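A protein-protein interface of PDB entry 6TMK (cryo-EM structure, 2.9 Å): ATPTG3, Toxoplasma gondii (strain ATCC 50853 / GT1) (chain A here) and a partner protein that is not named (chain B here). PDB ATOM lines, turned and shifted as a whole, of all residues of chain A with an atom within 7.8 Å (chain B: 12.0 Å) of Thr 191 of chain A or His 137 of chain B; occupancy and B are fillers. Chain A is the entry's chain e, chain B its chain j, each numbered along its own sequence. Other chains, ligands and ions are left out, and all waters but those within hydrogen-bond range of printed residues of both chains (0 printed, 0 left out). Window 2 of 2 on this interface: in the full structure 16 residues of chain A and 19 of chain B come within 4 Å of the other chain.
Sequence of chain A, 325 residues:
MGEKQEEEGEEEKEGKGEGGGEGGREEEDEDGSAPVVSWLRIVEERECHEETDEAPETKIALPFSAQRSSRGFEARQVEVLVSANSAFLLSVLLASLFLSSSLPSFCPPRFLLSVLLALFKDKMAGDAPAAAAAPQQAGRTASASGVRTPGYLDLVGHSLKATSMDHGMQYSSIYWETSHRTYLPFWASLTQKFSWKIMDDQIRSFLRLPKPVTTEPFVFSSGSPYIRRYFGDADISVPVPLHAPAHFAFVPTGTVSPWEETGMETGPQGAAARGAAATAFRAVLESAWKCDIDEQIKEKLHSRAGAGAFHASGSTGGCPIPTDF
The backbone carbonyl oxygen (O) of His 137 of chain B is in hydrogen-bond range of the side-chain amino group (NZ) of Lys 193 of chain A, 2.7 Å away.
O of Trp 187 of chain A lies within hydrogen-bond range of OG1 of Thr 191 of chain A (3.1 Å).
Tyr 183 of chain A touches Lys 129 of chain B (CD2 to CA, 3.7 Å). CD1 of Leu 133 of chain B touches O of Tyr 183 of chain A (3.7 Å). Leu 184 of chain A touches Phe 136 of chain B. Ala 188 of chain A touches Phe 136 of chain B. N of Ser 189 of chain A touches CZ of Phe 136 of chain B, at 3.8 Å. CE1 of His 137 of chain B touches CG2 of Thr 191 of chain A (3.8 Å).
Printed residues of chain B within 4 Å of Leu 184 of chain A: Phe 136 (3.9 Å). No residue of chain B comes within 4 Å of Pro 185 of chain A. Of the printed residues of chain B, Ser 189 of chain A touches Phe 136. No residue of chain B comes within 4 Å of Leu 190 of chain A. No residue of chain B comes within 4 Å of Gln 192 of chain A. Lys 193 of chain A touches just one residue of chain B: His 137. Trp 124 of chain B touches none of the printed residues of chain A. Printed residues of chain A within 4 Å of Phe 136 of chain B: Leu 184 (3.9 Å), Ala 188 (3.2 Å) and Ser 189 (3.8 Å). His 137 of chain B touches two residues of chain A. Gly 144 of chain B touches none of the printed residues of chain A. The nearest residue of chain B that does not touch Thr 191 of chain A is Phe 136 of chain B (5.7 Å). The nearest residue of chain A that does not touch His 137 of chain B is Ala 188 of chain A (4.2 Å).
Printed residues of chain B that touch a printed residue of chain A: Lys 129, Leu 133, Phe 136 and His 137. Hydrophobic or aromatic side chains of chain B that line the printed part of chain A: Leu 133, Phe 136 and His 137. Of the 11 printed residues of chain A, 6 touch a printed residue of chain B. Printed residues of chain A that touch a printed residue of chain B: Tyr 183, Leu 184, Ala 188, Ser 189, Thr 191 and Lys 193. Among the printed residues, 7 pairs touch across the chains.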
ATOM      1  N   TYR A 183       0.965  -0.147 -29.114  1.00  0.00           N
ATOM      2  CA  TYR A 183       1.430   0.699 -30.203  1.00  0.00           C
ATOM      3  C   TYR A 183       2.830   0.332 -30.669  1.00  0.00           C
ATOM      4  O   TYR A 183       3.512   1.153 -31.285  1.00  0.00           O
ATOM      5  CB  TYR A 183       1.379   2.181 -29.820  1.00  0.00           C
ATOM      6  CG  TYR A 183       0.041   2.658 -29.331  1.00  0.00           C
ATOM      7  CD1 TYR A 183      -1.012   2.837 -30.205  1.00  0.00           C
ATOM      8  CD2 TYR A 183      -0.168   2.939 -27.996  1.00  0.00           C
ATOM      9  CE1 TYR A 183      -2.228   3.275 -29.764  1.00  0.00           C
ATOM     10  CE2 TYR A 183      -1.383   3.376 -27.547  1.00  0.00           C
ATOM     11  CZ  TYR A 183      -2.410   3.546 -28.434  1.00  0.00           C
ATOM     12  OH  TYR A 183      -3.629   3.986 -27.986  1.00  0.00           O
ATOM     13  N   LEU A 184       3.275  -0.890 -30.397  1.00  0.00           N
ATOM     14  CA  LEU A 184       4.588  -1.348 -30.797  1.00  0.00           C
ATOM     15  C   LEU A 184       4.468  -2.598 -31.654  1.00  0.00           C
ATOM     16  O   LEU A 184       3.821  -3.566 -31.234  1.00  0.00           O
ATOM     17  CB  LEU A 184       5.449  -1.654 -29.571  1.00  0.00           C
ATOM     18  CG  LEU A 184       5.734  -0.536 -28.575  1.00  0.00           C
ATOM     19  CD1 LEU A 184       6.342  -1.124 -27.337  1.00  0.00           C
ATOM     20  CD2 LEU A 184       6.643   0.511 -29.154  1.00  0.00           C
ATOM     21  N   PRO A 185       5.055  -2.624 -32.848  1.00  0.00           N
ATOM     22  CA  PRO A 185       5.046  -3.855 -33.638  1.00  0.00           C
ATOM     23  C   PRO A 185       6.141  -4.829 -33.235  1.00  0.00           C
ATOM     24  O   PRO A 185       6.862  -4.594 -32.260  1.00  0.00           O
ATOM     25  CB  PRO A 185       5.249  -3.334 -35.060  1.00  0.00           C
ATOM     26  CG  PRO A 185       6.101  -2.159 -34.867  1.00  0.00           C
ATOM     27  CD  PRO A 185       5.574  -1.497 -33.634  1.00  0.00           C
ATOM     28  N   PHE A 186       6.280  -5.925 -33.978  1.00  0.00           N
ATOM     29  CA  PHE A 186       7.258  -6.950 -33.637  1.00  0.00           C
ATOM     30  C   PHE A 186       8.678  -6.628 -34.095  1.00  0.00           C
ATOM     31  O   PHE A 186       9.616  -7.270 -33.612  1.00  0.00           O
ATOM     32  CB  PHE A 186       6.802  -8.309 -34.190  1.00  0.00           C
ATOM     33  CG  PHE A 186       6.759  -8.391 -35.683  1.00  0.00           C
ATOM     34  CD1 PHE A 186       5.606  -8.073 -36.365  1.00  0.00           C
ATOM     35  CD2 PHE A 186       7.855  -8.817 -36.405  1.00  0.00           C
ATOM     36  CE1 PHE A 186       5.553  -8.154 -37.730  1.00  0.00           C
ATOM     37  CE2 PHE A 186       7.803  -8.896 -37.772  1.00  0.00           C
ATOM     38  CZ  PHE A 186       6.652  -8.564 -38.435  1.00  0.00           C
ATOM     39  N   TRP A 187       8.866  -5.657 -34.988  1.00  0.00           N
ATOM     40  CA  TRP A 187      10.191  -5.208 -35.405  1.00  0.00           C
ATOM     41  C   TRP A 187      10.634  -3.936 -34.690  1.00  0.00           C
ATOM     42  O   TRP A 187      11.603  -3.290 -35.118  1.00  0.00           O
ATOM     43  CB  TRP A 187      10.225  -4.990 -36.914  1.00  0.00           C
ATOM     44  CG  TRP A 187       9.352  -3.882 -37.391  1.00  0.00           C
ATOM     45  CD1 TRP A 187       9.678  -2.569 -37.459  1.00  0.00           C
ATOM     46  CD2 TRP A 187       8.013  -3.987 -37.874  1.00  0.00           C
ATOM     47  NE1 TRP A 187       8.629  -1.844 -37.950  1.00  0.00           N
ATOM     48  CE2 TRP A 187       7.592  -2.694 -38.213  1.00  0.00           C
ATOM     49  CE3 TRP A 187       7.128  -5.049 -38.049  1.00  0.00           C
ATOM     50  CZ2 TRP A 187       6.330  -2.433 -38.720  1.00  0.00           C
ATOM     51  CZ3 TRP A 187       5.879  -4.788 -38.551  1.00  0.00           C
ATOM     52  CH2 TRP A 187       5.489  -3.493 -38.881  1.00  0.00           C
ATOM     53  N   ALA A 188       9.959  -3.572 -33.604  1.00  0.00           N
ATOM     54  CA  ALA A 188      10.253  -2.323 -32.919  1.00  0.00           C
ATOM     55  C   ALA A 188      11.631  -2.337 -32.278  1.00  0.00           C
ATOM     56  O   ALA A 188      12.279  -1.290 -32.185  1.00  0.00           O
ATOM     57  CB  ALA A 188       9.179  -2.050 -31.873  1.00  0.00           C
ATOM     58  N   SER A 189      12.107  -3.505 -31.850  1.00  0.00           N
ATOM     59  CA  SER A 189      13.430  -3.575 -31.248  1.00  0.00           C
ATOM     60  C   SER A 189      14.520  -3.317 -32.277  1.00  0.00           C
ATOM     61  O   SER A 189      15.595  -2.820 -31.929  1.00  0.00           O
ATOM     62  CB  SER A 189      13.631  -4.928 -30.570  1.00  0.00           C
ATOM     63  OG  SER A 189      13.920  -5.943 -31.503  1.00  0.00           O
ATOM     64  N   LEU A 190      14.260  -3.635 -33.539  1.00  0.00           N
ATOM     65  CA  LEU A 190      15.204  -3.360 -34.609  1.00  0.00           C
ATOM     66  C   LEU A 190      15.060  -1.954 -35.161  1.00  0.00           C
ATOM     67  O   LEU A 190      16.018  -1.424 -35.734  1.00  0.00           O
ATOM     68  CB  LEU A 190      15.030  -4.376 -35.734  1.00  0.00           C
ATOM     69  CG  LEU A 190      14.959  -5.826 -35.274  1.00  0.00           C
ATOM     70  CD1 LEU A 190      14.729  -6.720 -36.459  1.00  0.00           C
ATOM     71  CD2 LEU A 190      16.228  -6.212 -34.541  1.00  0.00           C
ATOM     72  N   THR A 191      13.890  -1.344 -35.010  1.00  0.00           N
ATOM     73  CA  THR A 191      13.756   0.078 -35.290  1.00  0.00           C
ATOM     74  C   THR A 191      14.763   0.876 -34.468  1.00  0.00           C
ATOM     75  O   THR A 191      15.149   0.484 -33.366  1.00  0.00           O
ATOM     76  CB  THR A 191      12.342   0.556 -34.974  1.00  0.00           C
ATOM     77  OG1 THR A 191      11.388  -0.282 -35.635  1.00  0.00           O
ATOM     78  CG2 THR A 191      12.153   1.973 -35.440  1.00  0.00           C
ATOM     79  N   GLN A 192      15.205   2.002 -35.026  1.00  0.00           N
ATOM     80  CA  GLN A 192      16.033   2.942 -34.284  1.00  0.00           C
ATOM     81  C   GLN A 192      15.786   4.354 -34.793  1.00  0.00           C
ATOM     82  O   GLN A 192      15.298   4.562 -35.905  1.00  0.00           O
ATOM     83  CB  GLN A 192      17.519   2.597 -34.374  1.00  0.00           C
ATOM     84  CG  GLN A 192      18.088   2.615 -35.753  1.00  0.00           C
ATOM     85  CD  GLN A 192      19.530   2.171 -35.770  1.00  0.00           C
ATOM     86  OE1 GLN A 192      20.266   2.378 -34.807  1.00  0.00           O
ATOM     87  NE2 GLN A 192      19.941   1.551 -36.859  1.00  0.00           N
ATOM     88  N   LYS A 193      16.134   5.323 -33.952  1.00  0.00           N
ATOM     89  CA  LYS A 193      15.860   6.726 -34.211  1.00  0.00           C
ATOM     90  C   LYS A 193      16.868   7.306 -35.198  1.00  0.00           C
ATOM     91  O   LYS A 193      17.830   6.656 -35.613  1.00  0.00           O
ATOM     92  CB  LYS A 193      15.896   7.509 -32.905  1.00  0.00           C
ATOM     93  CG  LYS A 193      14.937   7.018 -31.863  1.00  0.00           C
ATOM     94  CD  LYS A 193      14.720   8.032 -30.765  1.00  0.00           C
ATOM     95  CE  LYS A 193      15.973   8.248 -29.952  1.00  0.00           C
ATOM     96  NZ  LYS A 193      16.572   7.028 -29.387  1.00  0.00           N
ATOM     97  N   TRP B 124      -0.750  15.622 -28.921  1.00  0.00           N
ATOM     98  CA  TRP B 124       0.207  14.563 -29.223  1.00  0.00           C
ATOM     99  C   TRP B 124       1.207  14.373 -28.093  1.00  0.00           C
ATOM    100  O   TRP B 124       1.576  13.238 -27.773  1.00  0.00           O
ATOM    101  CB  TRP B 124       0.943  14.865 -30.525  1.00  0.00           C
ATOM    102  CG  TRP B 124       2.035  13.898 -30.835  1.00  0.00           C
ATOM    103  CD1 TRP B 124       3.356  14.179 -30.948  1.00  0.00           C
ATOM    104  CD2 TRP B 124       1.907  12.493 -31.068  1.00  0.00           C
ATOM    105  NE1 TRP B 124       4.060  13.048 -31.231  1.00  0.00           N
ATOM    106  CE2 TRP B 124       3.193  11.997 -31.313  1.00  0.00           C
ATOM    107  CE3 TRP B 124       0.833  11.607 -31.093  1.00  0.00           C
ATOM    108  CZ2 TRP B 124       3.436  10.665 -31.574  1.00  0.00           C
ATOM    109  CZ3 TRP B 124       1.078  10.288 -31.355  1.00  0.00           C
ATOM    110  CH2 TRP B 124       2.364   9.828 -31.591  1.00  0.00           C
ATOM    111  N   PRO B 128      -0.710   8.510 -25.145  1.00  0.00           N
ATOM    112  CA  PRO B 128      -0.082   7.255 -24.719  1.00  0.00           C
ATOM    113  C   PRO B 128       0.856   6.674 -25.756  1.00  0.00           C
ATOM    114  O   PRO B 128       1.903   6.134 -25.390  1.00  0.00           O
ATOM    115  CB  PRO B 128      -1.289   6.345 -24.457  1.00  0.00           C
ATOM    116  CG  PRO B 128      -2.385   6.929 -25.230  1.00  0.00           C
ATOM    117  CD  PRO B 128      -2.170   8.388 -25.227  1.00  0.00           C
ATOM    118  N   LYS B 129       0.516   6.767 -27.040  1.00  0.00           N
ATOM    119  CA  LYS B 129       1.427   6.305 -28.078  1.00  0.00           C
ATOM    120  C   LYS B 129       2.753   7.046 -28.002  1.00  0.00           C
ATOM    121  O   LYS B 129       3.827   6.434 -28.023  1.00  0.00           O
ATOM    122  CB  LYS B 129       0.775   6.473 -29.445  1.00  0.00           C
ATOM    123  CG  LYS B 129       1.557   5.913 -30.594  1.00  0.00           C
ATOM    124  CD  LYS B 129       0.723   5.870 -31.835  1.00  0.00           C
ATOM    125  CE  LYS B 129       1.571   5.678 -33.058  1.00  0.00           C
ATOM    126  NZ  LYS B 129       2.229   4.361 -33.073  1.00  0.00           N
ATOM    127  N   PHE B 130       2.694   8.376 -27.911  1.00  0.00           N
ATOM    128  CA  PHE B 130       3.906   9.178 -27.832  1.00  0.00           C
ATOM    129  C   PHE B 130       4.730   8.813 -26.609  1.00  0.00           C
ATOM    130  O   PHE B 130       5.951   8.637 -26.697  1.00  0.00           O
ATOM    131  CB  PHE B 130       3.529  10.656 -27.819  1.00  0.00           C
ATOM    132  CG  PHE B 130       4.643  11.564 -27.447  1.00  0.00           C
ATOM    133  CD1 PHE B 130       4.643  12.196 -26.229  1.00  0.00           C
ATOM    134  CD2 PHE B 130       5.685  11.798 -28.307  1.00  0.00           C
ATOM    135  CE1 PHE B 130       5.652  13.025 -25.881  1.00  0.00           C
ATOM    136  CE2 PHE B 130       6.697  12.634 -27.954  1.00  0.00           C
ATOM    137  CZ  PHE B 130       6.681  13.247 -26.742  1.00  0.00           C
ATOM    138  N   ARG B 131       4.082   8.708 -25.450  1.00  0.00           N
ATOM    139  CA  ARG B 131       4.816   8.410 -24.231  1.00  0.00           C
ATOM    140  C   ARG B 131       5.461   7.033 -24.289  1.00  0.00           C
ATOM    141  O   ARG B 131       6.631   6.870 -23.919  1.00  0.00           O
ATOM    142  CB  ARG B 131       3.873   8.517 -23.041  1.00  0.00           C
ATOM    143  CG  ARG B 131       3.495   9.924 -22.695  1.00  0.00           C
ATOM    144  CD  ARG B 131       2.297   9.944 -21.811  1.00  0.00           C
ATOM    145  NE  ARG B 131       1.969  11.270 -21.314  1.00  0.00           N
ATOM    146  CZ  ARG B 131       0.799  11.581 -20.777  1.00  0.00           C
ATOM    147  NH1 ARG B 131      -0.146  10.671 -20.678  1.00  0.00           N
ATOM    148  NH2 ARG B 131       0.571  12.800 -20.336  1.00  0.00           N
ATOM    149  N   ILE B 132       4.718   6.030 -24.760  1.00  0.00           N
ATOM    150  CA  ILE B 132       5.262   4.681 -24.835  1.00  0.00           C
ATOM    151  C   ILE B 132       6.426   4.625 -25.812  1.00  0.00           C
ATOM    152  O   ILE B 132       7.443   3.982 -25.542  1.00  0.00           O
ATOM    153  CB  ILE B 132       4.152   3.676 -25.192  1.00  0.00           C
ATOM    154  CG1 ILE B 132       3.229   3.485 -23.997  1.00  0.00           C
ATOM    155  CG2 ILE B 132       4.735   2.360 -25.591  1.00  0.00           C
ATOM    156  CD1 ILE B 132       1.893   2.910 -24.329  1.00  0.00           C
ATOM    157  N   LEU B 133       6.295   5.282 -26.968  1.00  0.00           N
ATOM    158  CA  LEU B 133       7.377   5.274 -27.948  1.00  0.00           C
ATOM    159  C   LEU B 133       8.617   5.983 -27.429  1.00  0.00           C
ATOM    160  O   LEU B 133       9.742   5.525 -27.661  1.00  0.00           O
ATOM    161  CB  LEU B 133       6.919   5.900 -29.258  1.00  0.00           C
ATOM    162  CG  LEU B 133       6.433   4.948 -30.349  1.00  0.00           C
ATOM    163  CD1 LEU B 133       5.130   4.292 -30.042  1.00  0.00           C
ATOM    164  CD2 LEU B 133       6.312   5.731 -31.615  1.00  0.00           C
ATOM    165  N   SER B 134       8.438   7.100 -26.729  1.00  0.00           N
ATOM    166  CA  SER B 134       9.580   7.798 -26.158  1.00  0.00           C
ATOM    167  C   SER B 134      10.292   6.910 -25.149  1.00  0.00           C
ATOM    168  O   SER B 134      11.521   6.773 -25.178  1.00  0.00           O
ATOM    169  CB  SER B 134       9.119   9.103 -25.517  1.00  0.00           C
ATOM    170  OG  SER B 134       8.359   9.874 -26.417  1.00  0.00           O
ATOM    171  N   ALA B 135       9.528   6.280 -24.258  1.00  0.00           N
ATOM    172  CA  ALA B 135      10.125   5.395 -23.269  1.00  0.00           C
ATOM    173  C   ALA B 135      10.812   4.204 -23.927  1.00  0.00           C
ATOM    174  O   ALA B 135      11.867   3.757 -23.468  1.00  0.00           O
ATOM    175  CB  ALA B 135       9.053   4.929 -22.292  1.00  0.00           C
ATOM    176  N   PHE B 136      10.232   3.685 -25.009  1.00  0.00           N
ATOM    177  CA  PHE B 136      10.788   2.518 -25.681  1.00  0.00           C
ATOM    178  C   PHE B 136      12.096   2.847 -26.384  1.00  0.00           C
ATOM    179  O   PHE B 136      13.070   2.094 -26.285  1.00  0.00           O
ATOM    180  CB  PHE B 136       9.774   1.953 -26.675  1.00  0.00           C
ATOM    181  CG  PHE B 136      10.255   0.742 -27.401  1.00  0.00           C
ATOM    182  CD1 PHE B 136      10.196  -0.503 -26.816  1.00  0.00           C
ATOM    183  CD2 PHE B 136      10.781   0.848 -28.668  1.00  0.00           C
ATOM    184  CE1 PHE B 136      10.647  -1.604 -27.477  1.00  0.00           C
ATOM    185  CE2 PHE B 136      11.232  -0.249 -29.326  1.00  0.00           C
ATOM    186  CZ  PHE B 136      11.167  -1.480 -28.731  1.00  0.00           C
ATOM    187  N   HIS B 137      12.134   3.955 -27.115  1.00  0.00           N
ATOM    188  CA  HIS B 137      13.329   4.322 -27.856  1.00  0.00           C
ATOM    189  C   HIS B 137      14.347   5.069 -27.010  1.00  0.00           C
ATOM    190  O   HIS B 137      15.419   5.405 -27.519  1.00  0.00           O
ATOM    191  CB  HIS B 137      12.950   5.135 -29.089  1.00  0.00           C
ATOM    192  CG  HIS B 137      12.239   4.333 -30.130  1.00  0.00           C
ATOM    193  ND1 HIS B 137      12.881   3.400 -30.912  1.00  0.00           N
ATOM    194  CD2 HIS B 137      10.941   4.310 -30.507  1.00  0.00           C
ATOM    195  CE1 HIS B 137      12.009   2.840 -31.729  1.00  0.00           C
ATOM    196  NE2 HIS B 137      10.825   3.375 -31.504  1.00  0.00           N
ATOM    197  N   ASN B 138      14.045   5.329 -25.737  1.00  0.00           N
ATOM    198  CA  ASN B 138      15.038   5.749 -24.754  1.00  0.00           C
ATOM    199  C   ASN B 138      15.024   4.714 -23.634  1.00  0.00           C
ATOM    200  O   ASN B 138      14.381   4.911 -22.593  1.00  0.00           O
ATOM    201  CB  ASN B 138      14.746   7.152 -24.244  1.00  0.00           C
ATOM    202  CG  ASN B 138      14.825   8.182 -25.340  1.00  0.00           C
ATOM    203  OD1 ASN B 138      15.892   8.700 -25.655  1.00  0.00           O
ATOM    204  ND2 ASN B 138      13.693   8.462 -25.950  1.00  0.00           N
ATOM    205  N   PRO B 139      15.744   3.609 -23.810  1.00  0.00           N
ATOM    206  CA  PRO B 139      15.553   2.428 -22.959  1.00  0.00           C
ATOM    207  C   PRO B 139      15.638   2.648 -21.456  1.00  0.00           C
ATOM    208  O   PRO B 139      14.687   2.327 -20.737  1.00  0.00           O
ATOM    209  CB  PRO B 139      16.678   1.507 -23.437  1.00  0.00           C
ATOM    210  CG  PRO B 139      16.790   1.819 -24.859  1.00  0.00           C
ATOM    211  CD  PRO B 139      16.647   3.308 -24.928  1.00  0.00           C
ATOM    212  N   GLY B 140      16.753   3.163 -20.960  1.00  0.00           N
ATOM    213  CA  GLY B 140      16.945   3.221 -19.525  1.00  0.00           C
ATOM    214  C   GLY B 140      16.786   4.601 -18.934  1.00  0.00           C
ATOM    215  O   GLY B 140      17.352   4.896 -17.878  1.00  0.00           O
ATOM    216  N   LYS B 141      16.014   5.448 -19.594  1.00  0.00           N
ATOM    217  CA  LYS B 141      15.916   6.851 -19.242  1.00  0.00           C
ATOM    218  C   LYS B 141      14.466   7.226 -18.960  1.00  0.00           C
ATOM    219  O   LYS B 141      13.550   6.410 -19.064  1.00  0.00           O
ATOM    220  CB  LYS B 141      16.507   7.715 -20.353  1.00  0.00           C
ATOM    221  CG  LYS B 141      17.996   7.506 -20.547  1.00  0.00           C
ATOM    222  CD  LYS B 141      18.372   7.559 -21.999  1.00  0.00           C
ATOM    223  CE  LYS B 141      19.776   7.058 -22.229  1.00  0.00           C
ATOM    224  NZ  LYS B 141      20.770   7.820 -21.447  1.00  0.00           N
ATOM    225  N   ARG B 142      14.281   8.490 -18.593  1.00  0.00           N
ATOM    226  CA  ARG B 142      12.991   9.032 -18.175  1.00  0.00           C
ATOM    227  C   ARG B 142      12.721  10.293 -18.982  1.00  0.00           C
ATOM    228  O   ARG B 142      13.279  11.360 -18.672  1.00  0.00           O
ATOM    229  CB  ARG B 142      12.973   9.326 -16.686  1.00  0.00           C
ATOM    230  CG  ARG B 142      13.010   8.101 -15.819  1.00  0.00           C
ATOM    231  CD  ARG B 142      13.024   8.457 -14.363  1.00  0.00           C
ATOM    232  NE  ARG B 142      11.792   9.100 -13.932  1.00  0.00           N
ATOM    233  CZ  ARG B 142      10.673   8.458 -13.630  1.00  0.00           C
ATOM    234  NH1 ARG B 142       9.613   9.135 -13.246  1.00  0.00           N
ATOM    235  NH2 ARG B 142      10.610   7.145 -13.711  1.00  0.00           N
ATOM    236  N   PRO B 143      11.895  10.220 -20.014  1.00  0.00           N
ATOM    237  CA  PRO B 143      11.790  11.348 -20.944  1.00  0.00           C
ATOM    238  C   PRO B 143      10.785  12.418 -20.557  1.00  0.00           C
ATOM    239  O   PRO B 143      10.420  13.240 -21.400  1.00  0.00           O
ATOM    240  CB  PRO B 143      11.389  10.660 -22.253  1.00  0.00           C
ATOM    241  CG  PRO B 143      10.618   9.500 -21.821  1.00  0.00           C
ATOM    242  CD  PRO B 143      11.199   9.030 -20.533  1.00  0.00           C
ATOM    243  N   GLY B 144      10.335  12.439 -19.304  1.00  0.00           N
ATOM    244  CA  GLY B 144       9.410  13.480 -18.890  1.00  0.00           C
ATOM    245  C   GLY B 144       9.982  14.874 -19.068  1.00  0.00           C
ATOM    246  O   GLY B 144       9.287  15.795 -19.503  1.00  0.00           O
ATOM    247  N   LYS B 146      12.512  15.897 -21.138  1.00  0.00           N
ATOM    248  CA  LYS B 146      12.614  16.220 -22.551  1.00  0.00           C
ATOM    249  C   LYS B 146      11.248  16.485 -23.162  1.00  0.00           C
ATOM    250  O   LYS B 146      11.128  17.291 -24.087  1.00  0.00           O
ATOM    251  CB  LYS B 146      13.329  15.094 -23.290  1.00  0.00           C
ATOM    252  CG  LYS B 146      14.702  14.786 -22.770  1.00  0.00           C
ATOM    253  CD  LYS B 146      15.621  15.991 -22.821  1.00  0.00           C
ATOM    254  CE  LYS B 146      17.073  15.593 -22.617  1.00  0.00           C
ATOM    255  NZ  LYS B 146      18.025  16.680 -22.944  1.00  0.00           N
ATOM    256  N   ILE B 147      10.208  15.825 -22.659  1.00  0.00           N
ATOM    257  CA  ILE B 147       8.856  16.091 -23.132  1.00  0.00           C
ATOM    258  C   ILE B 147       8.416  17.492 -22.727  1.00  0.00           C
ATOM    259  O   ILE B 147       7.798  18.219 -23.515  1.00  0.00           O
ATOM    260  CB  ILE B 147       7.898  15.008 -22.613  1.00  0.00           C
ATOM    261  CG1 ILE B 147       8.176  13.699 -23.343  1.00  0.00           C
ATOM    262  CG2 ILE B 147       6.463  15.419 -22.823  1.00  0.00           C
ATOM    263  CD1 ILE B 147       7.666  12.486 -22.661  1.00  0.00           C
ATOM    264  N   MET B 150      10.099  19.782 -25.052  1.00  0.00           N
ATOM    265  CA  MET B 150       9.470  19.762 -26.365  1.00  0.00           C
ATOM    266  C   MET B 150       8.196  20.593 -26.363  1.00  0.00           C
ATOM    267  O   MET B 150       7.877  21.249 -27.356  1.00  0.00           O
ATOM    268  CB  MET B 150       9.154  18.329 -26.777  1.00  0.00           C
ATOM    269  CG  MET B 150      10.351  17.519 -27.177  1.00  0.00           C
ATOM    270  SD  MET B 150      10.033  15.751 -27.216  1.00  0.00           S
ATOM    271  CE  MET B 150       9.156  15.637 -28.767  1.00  0.00           C
